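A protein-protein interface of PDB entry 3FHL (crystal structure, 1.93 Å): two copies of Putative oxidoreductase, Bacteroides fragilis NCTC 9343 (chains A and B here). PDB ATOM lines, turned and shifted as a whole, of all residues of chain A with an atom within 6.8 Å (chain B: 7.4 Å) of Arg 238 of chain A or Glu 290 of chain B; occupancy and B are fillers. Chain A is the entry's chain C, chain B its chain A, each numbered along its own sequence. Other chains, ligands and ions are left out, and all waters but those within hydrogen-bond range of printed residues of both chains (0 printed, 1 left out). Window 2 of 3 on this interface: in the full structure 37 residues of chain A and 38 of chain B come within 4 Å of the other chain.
Of the printed residues of chain B, Tyr 156 of chain A touches Thr 249 and Leu 250.
Of the printed residues of chain A, Thr 249 of chain B touches Tyr 156 (2.6 Å) and Asn 158 (3.2 Å).
Of the printed residues of chain A, Glu 290 of chain B touches Arg 238.
The nearest residue of chain A that does not touch Glu 290 of chain B is Tyr 156 of chain A (5.4 Å).
No position is printed for both chains.
Of the 15 pairs that touch across the chains among the printed residues, none has its exchanged pair printed and touching as well.
Printed residues of chain B that touch a printed residue of chain A: His 247, Thr 249, Leu 250, Gly 251, Ser 252, His 288, Glu 290 and Glu 295.
Among the printed residues, Asp or Glu carboxylates within 4 Å of a Lys or Arg side-chain nitrogen of the other chain: Arg 238 of chain A with Glu 295 of chain B.
Among the printed residues, merely in contact across the chains: Glu 239 of chain A with His 247 of chain B (3.3 Å), Leu 236 of chain A with His 247 of chain B (3.3 Å), Tyr 156 of chain A with Leu 250 of chain B (3.5 Å), Arg 238 of chain A with His 288 of chain B (3.6 Å), Met 237 of chain A with His 247 of chain B (3.6 Å), Arg 238 of chain A with Glu 290 of chain B (3.7 Å), Arg 238 of chain A with Gly 251 of chain B (3.8 Å) and Met 237 of chain A with Ser 252 of chain B (3.9 Å).
OE1 of Glu 295 of chain B is in salt-bridge range of NH2 of Arg 238 of chain A (3.5 Å).
A ring nitrogen (ND1) of His 288 of chain B lies within hydrogen-bond range of the side-chain carboxylate of Glu 239 of chain A, 3.2 Å away.
The backbone carbonyl oxygen (O) of Thr 249 of chain B lies within hydrogen-bond range of the side-chain amide nitrogen (ND2) of Asn 158 of chain A, 3.2 Å away.
The guanidinium group (NH1) of Arg 238 of chain A lies within hydrogen-bond range of the backbone carbonyl oxygen (O) of Leu 250 of chain B (2.8 Å).
The side-chain hydroxyl of Tyr 156 of chain A is in hydrogen-bond range of the backbone carbonyl oxygen of Thr 249 of chain B (2.6 Å).
The backbone NH of Glu 239 of chain A sits at hydrogen-bond distance from the side-chain hydroxyl of Ser 252 of chain B, at 3.1 Å.
OG of Ser 252 of chain B lies within hydrogen-bond range of N of Arg 238 of chain A, at 3.1 Å.
The backbone carbonyl oxygen of Leu 250 of chain B lies within hydrogen-bond range of the backbone NH of Glu 290 of chain B (3.4 Å).
ND1 of His 288 of chain B sits at hydrogen-bond distance from SG of Cys 297 of chain B, 3.6 Å away.
The backbone carbonyl oxygen (O) of Arg 155 of chain A sits at hydrogen-bond distance from the backbone NH (N) of Leu 236 of chain A.
N of Ser 252 of chain B is in hydrogen-bond range of O of His 288 of chain B (2.8 Å).
O of Leu 143 of chain B is in hydrogen-bond range of N of Leu 250 of chain B.
O of Leu 250 of chain B is in hydrogen-bond range of OG1 of Thr 289 of chain B (3.3 Å).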
ATOM      1  N   ARG A 155      24.196   1.884  -5.729  1.00  0.00           N
ATOM      2  CA  ARG A 155      23.538   0.969  -6.655  1.00  0.00           C
ATOM      3  C   ARG A 155      23.765  -0.464  -6.196  1.00  0.00           C
ATOM      4  O   ARG A 155      24.632  -0.725  -5.375  1.00  0.00           O
ATOM      5  CB  ARG A 155      24.084   1.165  -8.079  1.00  0.00           C
ATOM      6  CG  ARG A 155      23.783   2.540  -8.683  1.00  0.00           C
ATOM      7  CD  ARG A 155      23.928   2.541 -10.199  1.00  0.00           C
ATOM      8  NE  ARG A 155      23.398   3.766 -10.800  1.00  0.00           N
ATOM      9  CZ  ARG A 155      23.588   4.139 -12.065  1.00  0.00           C
ATOM     10  NH1 ARG A 155      24.314   3.389 -12.890  1.00  0.00           N
ATOM     11  NH2 ARG A 155      23.057   5.277 -12.500  1.00  0.00           N
ATOM     12  N   TYR A 156      22.977  -1.391  -6.725  1.00  0.00           N
ATOM     13  CA  TYR A 156      23.179  -2.792  -6.437  1.00  0.00           C
ATOM     14  C   TYR A 156      22.948  -3.624  -7.688  1.00  0.00           C
ATOM     15  O   TYR A 156      21.808  -3.863  -8.077  1.00  0.00           O
ATOM     16  CB  TYR A 156      22.298  -3.284  -5.264  1.00  0.00           C
ATOM     17  CG  TYR A 156      22.543  -4.747  -4.946  1.00  0.00           C
ATOM     18  CD1 TYR A 156      23.726  -5.155  -4.323  1.00  0.00           C
ATOM     19  CD2 TYR A 156      21.622  -5.730  -5.317  1.00  0.00           C
ATOM     20  CE1 TYR A 156      23.971  -6.495  -4.061  1.00  0.00           C
ATOM     21  CE2 TYR A 156      21.862  -7.070  -5.076  1.00  0.00           C
ATOM     22  CZ  TYR A 156      23.042  -7.447  -4.443  1.00  0.00           C
ATOM     23  OH  TYR A 156      23.296  -8.773  -4.193  1.00  0.00           O
ATOM     24  N   ASN A 158      24.892  -7.135  -8.756  1.00  0.00           N
ATOM     25  CA  ASN A 158      25.914  -8.131  -8.503  1.00  0.00           C
ATOM     26  C   ASN A 158      26.042  -9.052  -9.670  1.00  0.00           C
ATOM     27  O   ASN A 158      25.847 -10.220  -9.550  1.00  0.00           O
ATOM     28  CB  ASN A 158      25.575  -8.941  -7.266  1.00  0.00           C
ATOM     29  CG  ASN A 158      26.644  -9.934  -6.902  1.00  0.00           C
ATOM     30  OD1 ASN A 158      27.810  -9.709  -7.115  1.00  0.00           O
ATOM     31  ND2 ASN A 158      26.240 -11.029  -6.338  1.00  0.00           N
ATOM     32  N   TYR A 235      28.490  -0.303  -6.966  1.00  0.00           N
ATOM     33  CA  TYR A 235      27.503  -1.244  -7.487  1.00  0.00           C
ATOM     34  C   TYR A 235      27.152  -2.349  -6.489  1.00  0.00           C
ATOM     35  O   TYR A 235      26.380  -3.249  -6.805  1.00  0.00           O
ATOM     36  CB  TYR A 235      27.986  -1.854  -8.800  1.00  0.00           C
ATOM     37  CG  TYR A 235      27.563  -1.076 -10.024  1.00  0.00           C
ATOM     38  CD1 TYR A 235      26.216  -0.944 -10.359  1.00  0.00           C
ATOM     39  CD2 TYR A 235      28.508  -0.486 -10.854  1.00  0.00           C
ATOM     40  CE1 TYR A 235      25.824  -0.244 -11.488  1.00  0.00           C
ATOM     41  CE2 TYR A 235      28.126   0.211 -11.993  1.00  0.00           C
ATOM     42  CZ  TYR A 235      26.784   0.338 -12.297  1.00  0.00           C
ATOM     43  OH  TYR A 235      26.409   1.045 -13.419  1.00  0.00           O
ATOM     44  N   LEU A 236      27.704  -2.275  -5.282  1.00  0.00           N
ATOM     45  CA  LEU A 236      27.354  -3.242  -4.242  1.00  0.00           C
ATOM     46  C   LEU A 236      26.932  -2.568  -2.947  1.00  0.00           C
ATOM     47  O   LEU A 236      27.678  -2.558  -1.960  1.00  0.00           O
ATOM     48  CB  LEU A 236      28.513  -4.217  -4.009  1.00  0.00           C
ATOM     49  CG  LEU A 236      28.749  -5.280  -5.088  1.00  0.00           C
ATOM     50  CD1 LEU A 236      29.964  -6.122  -4.672  1.00  0.00           C
ATOM     51  CD2 LEU A 236      27.500  -6.159  -5.311  1.00  0.00           C
ATOM     52  N   MET A 237      25.758  -1.945  -2.986  1.00  0.00           N
ATOM     53  CA  MET A 237      25.145  -1.323  -1.817  1.00  0.00           C
ATOM     54  C   MET A 237      23.674  -1.709  -1.832  1.00  0.00           C
ATOM     55  O   MET A 237      22.809  -0.897  -2.201  1.00  0.00           O
ATOM     56  CB  MET A 237      25.280   0.216  -1.810  1.00  0.00           C
ATOM     57  CG  MET A 237      26.674   0.780  -1.656  1.00  0.00           C
ATOM     58  SD  MET A 237      26.730   2.588  -1.497  1.00  0.00           S
ATOM     59  CE  MET A 237      28.445   2.811  -1.059  1.00  0.00           C
ATOM     60  N   ARG A 238      23.391  -2.955  -1.447  1.00  0.00           N
ATOM     61  CA  ARG A 238      22.015  -3.470  -1.454  1.00  0.00           C
ATOM     62  C   ARG A 238      21.074  -2.602  -0.651  1.00  0.00           C
ATOM     63  O   ARG A 238      19.942  -2.351  -1.067  1.00  0.00           O
ATOM     64  CB  ARG A 238      21.923  -4.941  -1.014  1.00  0.00           C
ATOM     65  CG  ARG A 238      20.587  -5.548  -1.445  1.00  0.00           C
ATOM     66  CD  ARG A 238      20.576  -7.042  -1.471  1.00  0.00           C
ATOM     67  NE  ARG A 238      19.484  -7.512  -2.315  1.00  0.00           N
ATOM     68  CZ  ARG A 238      19.363  -8.751  -2.788  1.00  0.00           C
ATOM     69  NH1 ARG A 238      20.264  -9.677  -2.502  1.00  0.00           N
ATOM     70  NH2 ARG A 238      18.333  -9.063  -3.562  1.00  0.00           N
ATOM     71  N   GLU A 239      21.545  -2.135   0.501  1.00  0.00           N
ATOM     72  CA  GLU A 239      20.839  -1.109   1.222  1.00  0.00           C
ATOM     73  C   GLU A 239      21.602   0.190   0.968  1.00  0.00           C
ATOM     74  O   GLU A 239      22.781   0.311   1.297  1.00  0.00           O
ATOM     75  CB  GLU A 239      20.748  -1.432   2.707  1.00  0.00           C
ATOM     76  CG  GLU A 239      20.024  -0.369   3.533  1.00  0.00           C
ATOM     77  CD  GLU A 239      18.532  -0.272   3.233  1.00  0.00           C
ATOM     78  OE1 GLU A 239      17.949  -1.209   2.628  1.00  0.00           O
ATOM     79  OE2 GLU A 239      17.944   0.753   3.634  1.00  0.00           O
ATOM     80  N   ALA A 240      20.909   1.136   0.349  1.00  0.00           N
ATOM     81  CA  ALA A 240      21.522   2.322  -0.179  1.00  0.00           C
ATOM     82  C   ALA A 240      21.970   3.253   0.929  1.00  0.00           C
ATOM     83  O   ALA A 240      21.251   3.478   1.897  1.00  0.00           O
ATOM     84  CB  ALA A 240      20.541   3.041  -1.112  1.00  0.00           C
ATOM     85  N   SER B 141      28.483 -15.345   7.230  1.00  0.00           N
ATOM     86  CA  SER B 141      28.502 -14.880   5.822  1.00  0.00           C
ATOM     87  C   SER B 141      27.129 -14.452   5.291  1.00  0.00           C
ATOM     88  O   SER B 141      26.781 -14.770   4.149  1.00  0.00           O
ATOM     89  CB  SER B 141      29.120 -15.932   4.886  1.00  0.00           C
ATOM     90  OG  SER B 141      30.476 -16.186   5.199  1.00  0.00           O
ATOM     91  N   LEU B 142      26.354 -13.746   6.122  1.00  0.00           N
ATOM     92  CA  LEU B 142      24.985 -13.354   5.766  1.00  0.00           C
ATOM     93  C   LEU B 142      24.942 -12.388   4.576  1.00  0.00           C
ATOM     94  O   LEU B 142      23.972 -12.373   3.819  1.00  0.00           O
ATOM     95  CB  LEU B 142      24.221 -12.791   6.978  1.00  0.00           C
ATOM     96  CG  LEU B 142      23.978 -13.727   8.175  1.00  0.00           C
ATOM     97  CD1 LEU B 142      23.167 -13.042   9.249  1.00  0.00           C
ATOM     98  CD2 LEU B 142      23.274 -15.016   7.752  1.00  0.00           C
ATOM     99  N   LEU B 143      26.031 -11.645   4.384  1.00  0.00           N
ATOM    100  CA  LEU B 143      26.128 -10.641   3.336  1.00  0.00           C
ATOM    101  C   LEU B 143      26.822 -11.171   2.087  1.00  0.00           C
ATOM    102  O   LEU B 143      27.089 -10.417   1.151  1.00  0.00           O
ATOM    103  CB  LEU B 143      26.882  -9.418   3.888  1.00  0.00           C
ATOM    104  CG  LEU B 143      26.167  -8.335   4.697  1.00  0.00           C
ATOM    105  CD1 LEU B 143      24.816  -8.707   5.274  1.00  0.00           C
ATOM    106  CD2 LEU B 143      27.072  -7.780   5.757  1.00  0.00           C
ATOM    107  N   GLY B 144      27.101 -12.472   2.055  1.00  0.00           N
ATOM    108  CA  GLY B 144      27.942 -13.034   1.009  1.00  0.00           C
ATOM    109  C   GLY B 144      29.397 -12.730   1.278  1.00  0.00           C
ATOM    110  O   GLY B 144      29.859 -12.854   2.408  1.00  0.00           O
ATOM    111  N   LEU B 246      27.683  -2.280   6.578  1.00  0.00           N
ATOM    112  CA  LEU B 246      28.455  -3.319   5.946  1.00  0.00           C
ATOM    113  C   LEU B 246      27.805  -3.691   4.642  1.00  0.00           C
ATOM    114  O   LEU B 246      26.592  -3.804   4.593  1.00  0.00           O
ATOM    115  CB  LEU B 246      28.493  -4.549   6.857  1.00  0.00           C
ATOM    116  CG  LEU B 246      29.574  -4.602   7.943  1.00  0.00           C
ATOM    117  CD1 LEU B 246      29.363  -3.608   9.075  1.00  0.00           C
ATOM    118  CD2 LEU B 246      29.635  -6.011   8.501  1.00  0.00           C
ATOM    119  N   HIS B 247      28.607  -3.871   3.597  1.00  0.00           N
ATOM    120  CA  HIS B 247      28.099  -4.261   2.289  1.00  0.00           C
ATOM    121  C   HIS B 247      28.838  -5.478   1.793  1.00  0.00           C
ATOM    122  O   HIS B 247      30.066  -5.563   1.845  1.00  0.00           O
ATOM    123  CB  HIS B 247      28.239  -3.134   1.239  1.00  0.00           C
ATOM    124  CG  HIS B 247      27.538  -1.869   1.615  1.00  0.00           C
ATOM    125  ND1 HIS B 247      26.165  -1.764   1.657  1.00  0.00           N
ATOM    126  CD2 HIS B 247      28.019  -0.660   1.988  1.00  0.00           C
ATOM    127  CE1 HIS B 247      25.828  -0.547   2.041  1.00  0.00           C
ATOM    128  NE2 HIS B 247      26.934   0.143   2.254  1.00  0.00           N
ATOM    129  N   GLY B 248      28.069  -6.434   1.312  1.00  0.00           N
ATOM    130  CA  GLY B 248      28.648  -7.577   0.650  1.00  0.00           C
ATOM    131  C   GLY B 248      28.017  -7.824  -0.699  1.00  0.00           C
ATOM    132  O   GLY B 248      27.164  -7.058  -1.158  1.00  0.00           O
ATOM    133  N   THR B 249      28.434  -8.910  -1.334  1.00  0.00           N
ATOM    134  CA  THR B 249      27.942  -9.274  -2.660  1.00  0.00           C
ATOM    135  C   THR B 249      26.457  -9.623  -2.653  1.00  0.00           C
ATOM    136  O   THR B 249      25.765  -9.408  -3.637  1.00  0.00           O
ATOM    137  CB  THR B 249      28.738 -10.459  -3.243  1.00  0.00           C
ATOM    138  OG1 THR B 249      28.735 -11.539  -2.305  1.00  0.00           O
ATOM    139  CG2 THR B 249      30.172 -10.043  -3.545  1.00  0.00           C
ATOM    140  N   LEU B 250      25.968 -10.135  -1.529  1.00  0.00           N
ATOM    141  CA  LEU B 250      24.581 -10.570  -1.415  1.00  0.00           C
ATOM    142  C   LEU B 250      23.697  -9.594  -0.648  1.00  0.00           C
ATOM    143  O   LEU B 250      22.471  -9.684  -0.701  1.00  0.00           O
ATOM    144  CB  LEU B 250      24.529 -11.953  -0.746  1.00  0.00           C
ATOM    145  CG  LEU B 250      24.299 -13.231  -1.564  1.00  0.00           C
ATOM    146  CD1 LEU B 250      24.749 -13.136  -3.021  1.00  0.00           C
ATOM    147  CD2 LEU B 250      24.928 -14.440  -0.858  1.00  0.00           C
ATOM    148  N   GLY B 251      24.300  -8.670   0.093  1.00  0.00           N
ATOM    149  CA  GLY B 251      23.483  -7.797   0.904  1.00  0.00           C
ATOM    150  C   GLY B 251      24.223  -6.827   1.795  1.00  0.00           C
ATOM    151  O   GLY B 251      25.442  -6.708   1.722  1.00  0.00           O
ATOM    152  N   SER B 252      23.455  -6.156   2.646  1.00  0.00           N
ATOM    153  CA  SER B 252      23.973  -5.083   3.486  1.00  0.00           C
ATOM    154  C   SER B 252      23.399  -5.197   4.880  1.00  0.00           C
ATOM    155  O   SER B 252      22.312  -5.756   5.077  1.00  0.00           O
ATOM    156  CB  SER B 252      23.594  -3.710   2.896  1.00  0.00           C
ATOM    157  OG  SER B 252      24.046  -3.545   1.549  1.00  0.00           O
ATOM    158  N   TYR B 253      24.119  -4.644   5.848  1.00  0.00           N
ATOM    159  CA  TYR B 253      23.621  -4.547   7.209  1.00  0.00           C
ATOM    160  C   TYR B 253      23.888  -3.119   7.668  1.00  0.00           C
ATOM    161  O   TYR B 253      25.002  -2.635   7.529  1.00  0.00           O
ATOM    162  CB  TYR B 253      24.322  -5.568   8.127  1.00  0.00           C
ATOM    163  CG  TYR B 253      24.000  -5.387   9.592  1.00  0.00           C
ATOM    164  CD1 TYR B 253      22.764  -5.771  10.097  1.00  0.00           C
ATOM    165  CD2 TYR B 253      24.930  -4.825  10.473  1.00  0.00           C
ATOM    166  CE1 TYR B 253      22.449  -5.602  11.440  1.00  0.00           C
ATOM    167  CE2 TYR B 253      24.619  -4.652  11.825  1.00  0.00           C
ATOM    168  CZ  TYR B 253      23.385  -5.059  12.294  1.00  0.00           C
ATOM    169  OH  TYR B 253      23.063  -4.898  13.611  1.00  0.00           O
ATOM    170  N   LEU B 287      18.820  -5.741   8.154  1.00  0.00           N
ATOM    171  CA  LEU B 287      19.511  -6.732   7.372  1.00  0.00           C
ATOM    172  C   LEU B 287      18.773  -6.869   6.051  1.00  0.00           C
ATOM    173  O   LEU B 287      17.606  -7.223   6.016  1.00  0.00           O
ATOM    174  CB  LEU B 287      19.538  -8.077   8.107  1.00  0.00           C
ATOM    175  CG  LEU B 287      20.185  -9.248   7.377  1.00  0.00           C
ATOM    176  CD1 LEU B 287      21.690  -8.991   7.186  1.00  0.00           C
ATOM    177  CD2 LEU B 287      19.954 -10.554   8.139  1.00  0.00           C
ATOM    178  N   HIS B 288      19.466  -6.586   4.967  1.00  0.00           N
ATOM    179  CA  HIS B 288      18.851  -6.647   3.659  1.00  0.00           C
ATOM    180  C   HIS B 288      19.759  -7.498   2.805  1.00  0.00           C
ATOM    181  O   HIS B 288      20.771  -7.025   2.317  1.00  0.00           O
ATOM    182  CB  HIS B 288      18.685  -5.232   3.079  1.00  0.00           C
ATOM    183  CG  HIS B 288      17.972  -5.195   1.756  1.00  0.00           C
ATOM    184  ND1 HIS B 288      17.596  -4.017   1.153  1.00  0.00           N
ATOM    185  CD2 HIS B 288      17.556  -6.187   0.930  1.00  0.00           C
ATOM    186  CE1 HIS B 288      16.995  -4.280   0.006  1.00  0.00           C
ATOM    187  NE2 HIS B 288      16.958  -5.590  -0.153  1.00  0.00           N
ATOM    188  N   THR B 289      19.392  -8.762   2.619  1.00  0.00           N
ATOM    189  CA  THR B 289      20.300  -9.713   1.991  1.00  0.00           C
ATOM    190  C   THR B 289      19.530 -10.853   1.313  1.00  0.00           C
ATOM    191  O   THR B 289      18.301 -10.826   1.241  1.00  0.00           O
ATOM    192  CB  THR B 289      21.388 -10.239   3.022  1.00  0.00           C
ATOM    193  OG1 THR B 289      22.409 -10.949   2.322  1.00  0.00           O
ATOM    194  CG2 THR B 289      20.781 -11.135   4.098  1.00  0.00           C
ATOM    195  N   GLU B 290      20.266 -11.822   0.793  1.00  0.00           N
ATOM    196  CA  GLU B 290      19.692 -12.999   0.161  1.00  0.00           C
ATOM    197  C   GLU B 290      19.959 -14.224   1.038  1.00  0.00           C
ATOM    198  O   GLU B 290      21.112 -14.534   1.359  1.00  0.00           O
ATOM    199  CB  GLU B 290      20.348 -13.180  -1.201  1.00  0.00           C
ATOM    200  CG  GLU B 290      19.763 -14.256  -2.088  1.00  0.00           C
ATOM    201  CD  GLU B 290      20.548 -14.387  -3.391  1.00  0.00           C
ATOM    202  OE1 GLU B 290      20.594 -13.394  -4.158  1.00  0.00           O
ATOM    203  OE2 GLU B 290      21.124 -15.474  -3.640  1.00  0.00           O
ATOM    204  N   ILE B 291      18.895 -14.914   1.435  1.00  0.00           N
ATOM    205  CA  ILE B 291      19.024 -16.107   2.268  1.00  0.00           C
ATOM    206  C   ILE B 291      18.281 -17.260   1.604  1.00  0.00           C
ATOM    207  O   ILE B 291      17.074 -17.151   1.333  1.00  0.00           O
ATOM    208  CB  ILE B 291      18.490 -15.866   3.696  1.00  0.00           C
ATOM    209  CG1 ILE B 291      19.335 -14.792   4.396  1.00  0.00           C
ATOM    210  CG2 ILE B 291      18.490 -17.165   4.503  1.00  0.00           C
ATOM    211  CD1 ILE B 291      18.904 -14.465   5.798  1.00  0.00           C
ATOM    212  N   ASN B 292      19.013 -18.347   1.344  1.00  0.00           N
ATOM    213  CA  ASN B 292      18.507 -19.522   0.621  1.00  0.00           C
ATOM    214  C   ASN B 292      17.855 -19.113  -0.710  1.00  0.00           C
ATOM    215  O   ASN B 292      16.767 -19.587  -1.062  1.00  0.00           O
ATOM    216  CB  ASN B 292      17.540 -20.351   1.502  1.00  0.00           C
ATOM    217  CG  ASN B 292      18.216 -20.948   2.744  1.00  0.00           C
ATOM    218  OD1 ASN B 292      19.364 -21.380   2.695  1.00  0.00           O
ATOM    219  ND2 ASN B 292      17.492 -20.977   3.853  1.00  0.00           N
ATOM    220  N   GLY B 293      18.516 -18.192  -1.416  1.00  0.00           N
ATOM    221  CA  GLY B 293      18.040 -17.678  -2.698  1.00  0.00           C
ATOM    222  C   GLY B 293      16.843 -16.738  -2.680  1.00  0.00           C
ATOM    223  O   GLY B 293      16.284 -16.435  -3.736  1.00  0.00           O
ATOM    224  N   LYS B 294      16.444 -16.273  -1.497  1.00  0.00           N
ATOM    225  CA  LYS B 294      15.304 -15.365  -1.366  1.00  0.00           C
ATOM    226  C   LYS B 294      15.727 -14.044  -0.727  1.00  0.00           C
ATOM    227  O   LYS B 294      16.432 -14.039   0.280  1.00  0.00           O
ATOM    228  CB  LYS B 294      14.194 -16.011  -0.528  1.00  0.00           C
ATOM    229  CG  LYS B 294      13.668 -17.338  -1.083  1.00  0.00           C
ATOM    230  CD  LYS B 294      12.406 -17.785  -0.363  1.00  0.00           C
ATOM    231  CE  LYS B 294      11.831 -19.053  -0.989  1.00  0.00           C
ATOM    232  NZ  LYS B 294      11.610 -18.909  -2.461  1.00  0.00           N
ATOM    233  N   GLU B 295      15.293 -12.928  -1.310  1.00  0.00           N
ATOM    234  CA  GLU B 295      15.589 -11.612  -0.751  1.00  0.00           C
ATOM    235  C   GLU B 295      14.834 -11.410   0.553  1.00  0.00           C
ATOM    236  O   GLU B 295      13.630 -11.652   0.633  1.00  0.00           O
ATOM    237  CB  GLU B 295      15.249 -10.492  -1.744  1.00  0.00           C
ATOM    238  CG  GLU B 295      15.524  -9.074  -1.215  1.00  0.00           C
ATOM    239  CD  GLU B 295      15.234  -7.974  -2.236  1.00  0.00           C
ATOM    240  OE1 GLU B 295      14.889  -8.296  -3.397  1.00  0.00           O
ATOM    241  OE2 GLU B 295      15.364  -6.780  -1.874  1.00  0.00           O
ATOM    242  N   ILE B 296      15.560 -11.000   1.589  1.00  0.00           N
ATOM    243  CA  ILE B 296      14.941 -10.618   2.846  1.00  0.00           C
ATOM    244  C   ILE B 296      15.379  -9.199   3.200  1.00  0.00           C
ATOM    245  O   ILE B 296      16.503  -8.801   2.913  1.00  0.00           O
ATOM    246  CB  ILE B 296      15.227 -11.645   4.011  1.00  0.00           C
ATOM    247  CG1 ILE B 296      16.709 -11.691   4.402  1.00  0.00           C
ATOM    248  CG2 ILE B 296      14.730 -13.055   3.659  1.00  0.00           C
ATOM    249  CD1 ILE B 296      17.037 -10.897   5.656  1.00  0.00           C
ATOM    250  N   CYS B 297      14.480  -8.439   3.802  1.00  0.00           N
ATOM    251  CA  CYS B 297      14.780  -7.086   4.240  1.00  0.00           C
ATOM    252  C   CYS B 297      14.012  -6.865   5.533  1.00  0.00           C
ATOM    253  O   CYS B 297      12.813  -6.587   5.513  1.00  0.00           O
ATOM    254  CB  CYS B 297      14.390  -6.068   3.160  1.00  0.00           C
ATOM    255  SG  CYS B 297      14.891  -4.366   3.525  1.00  0.00           S
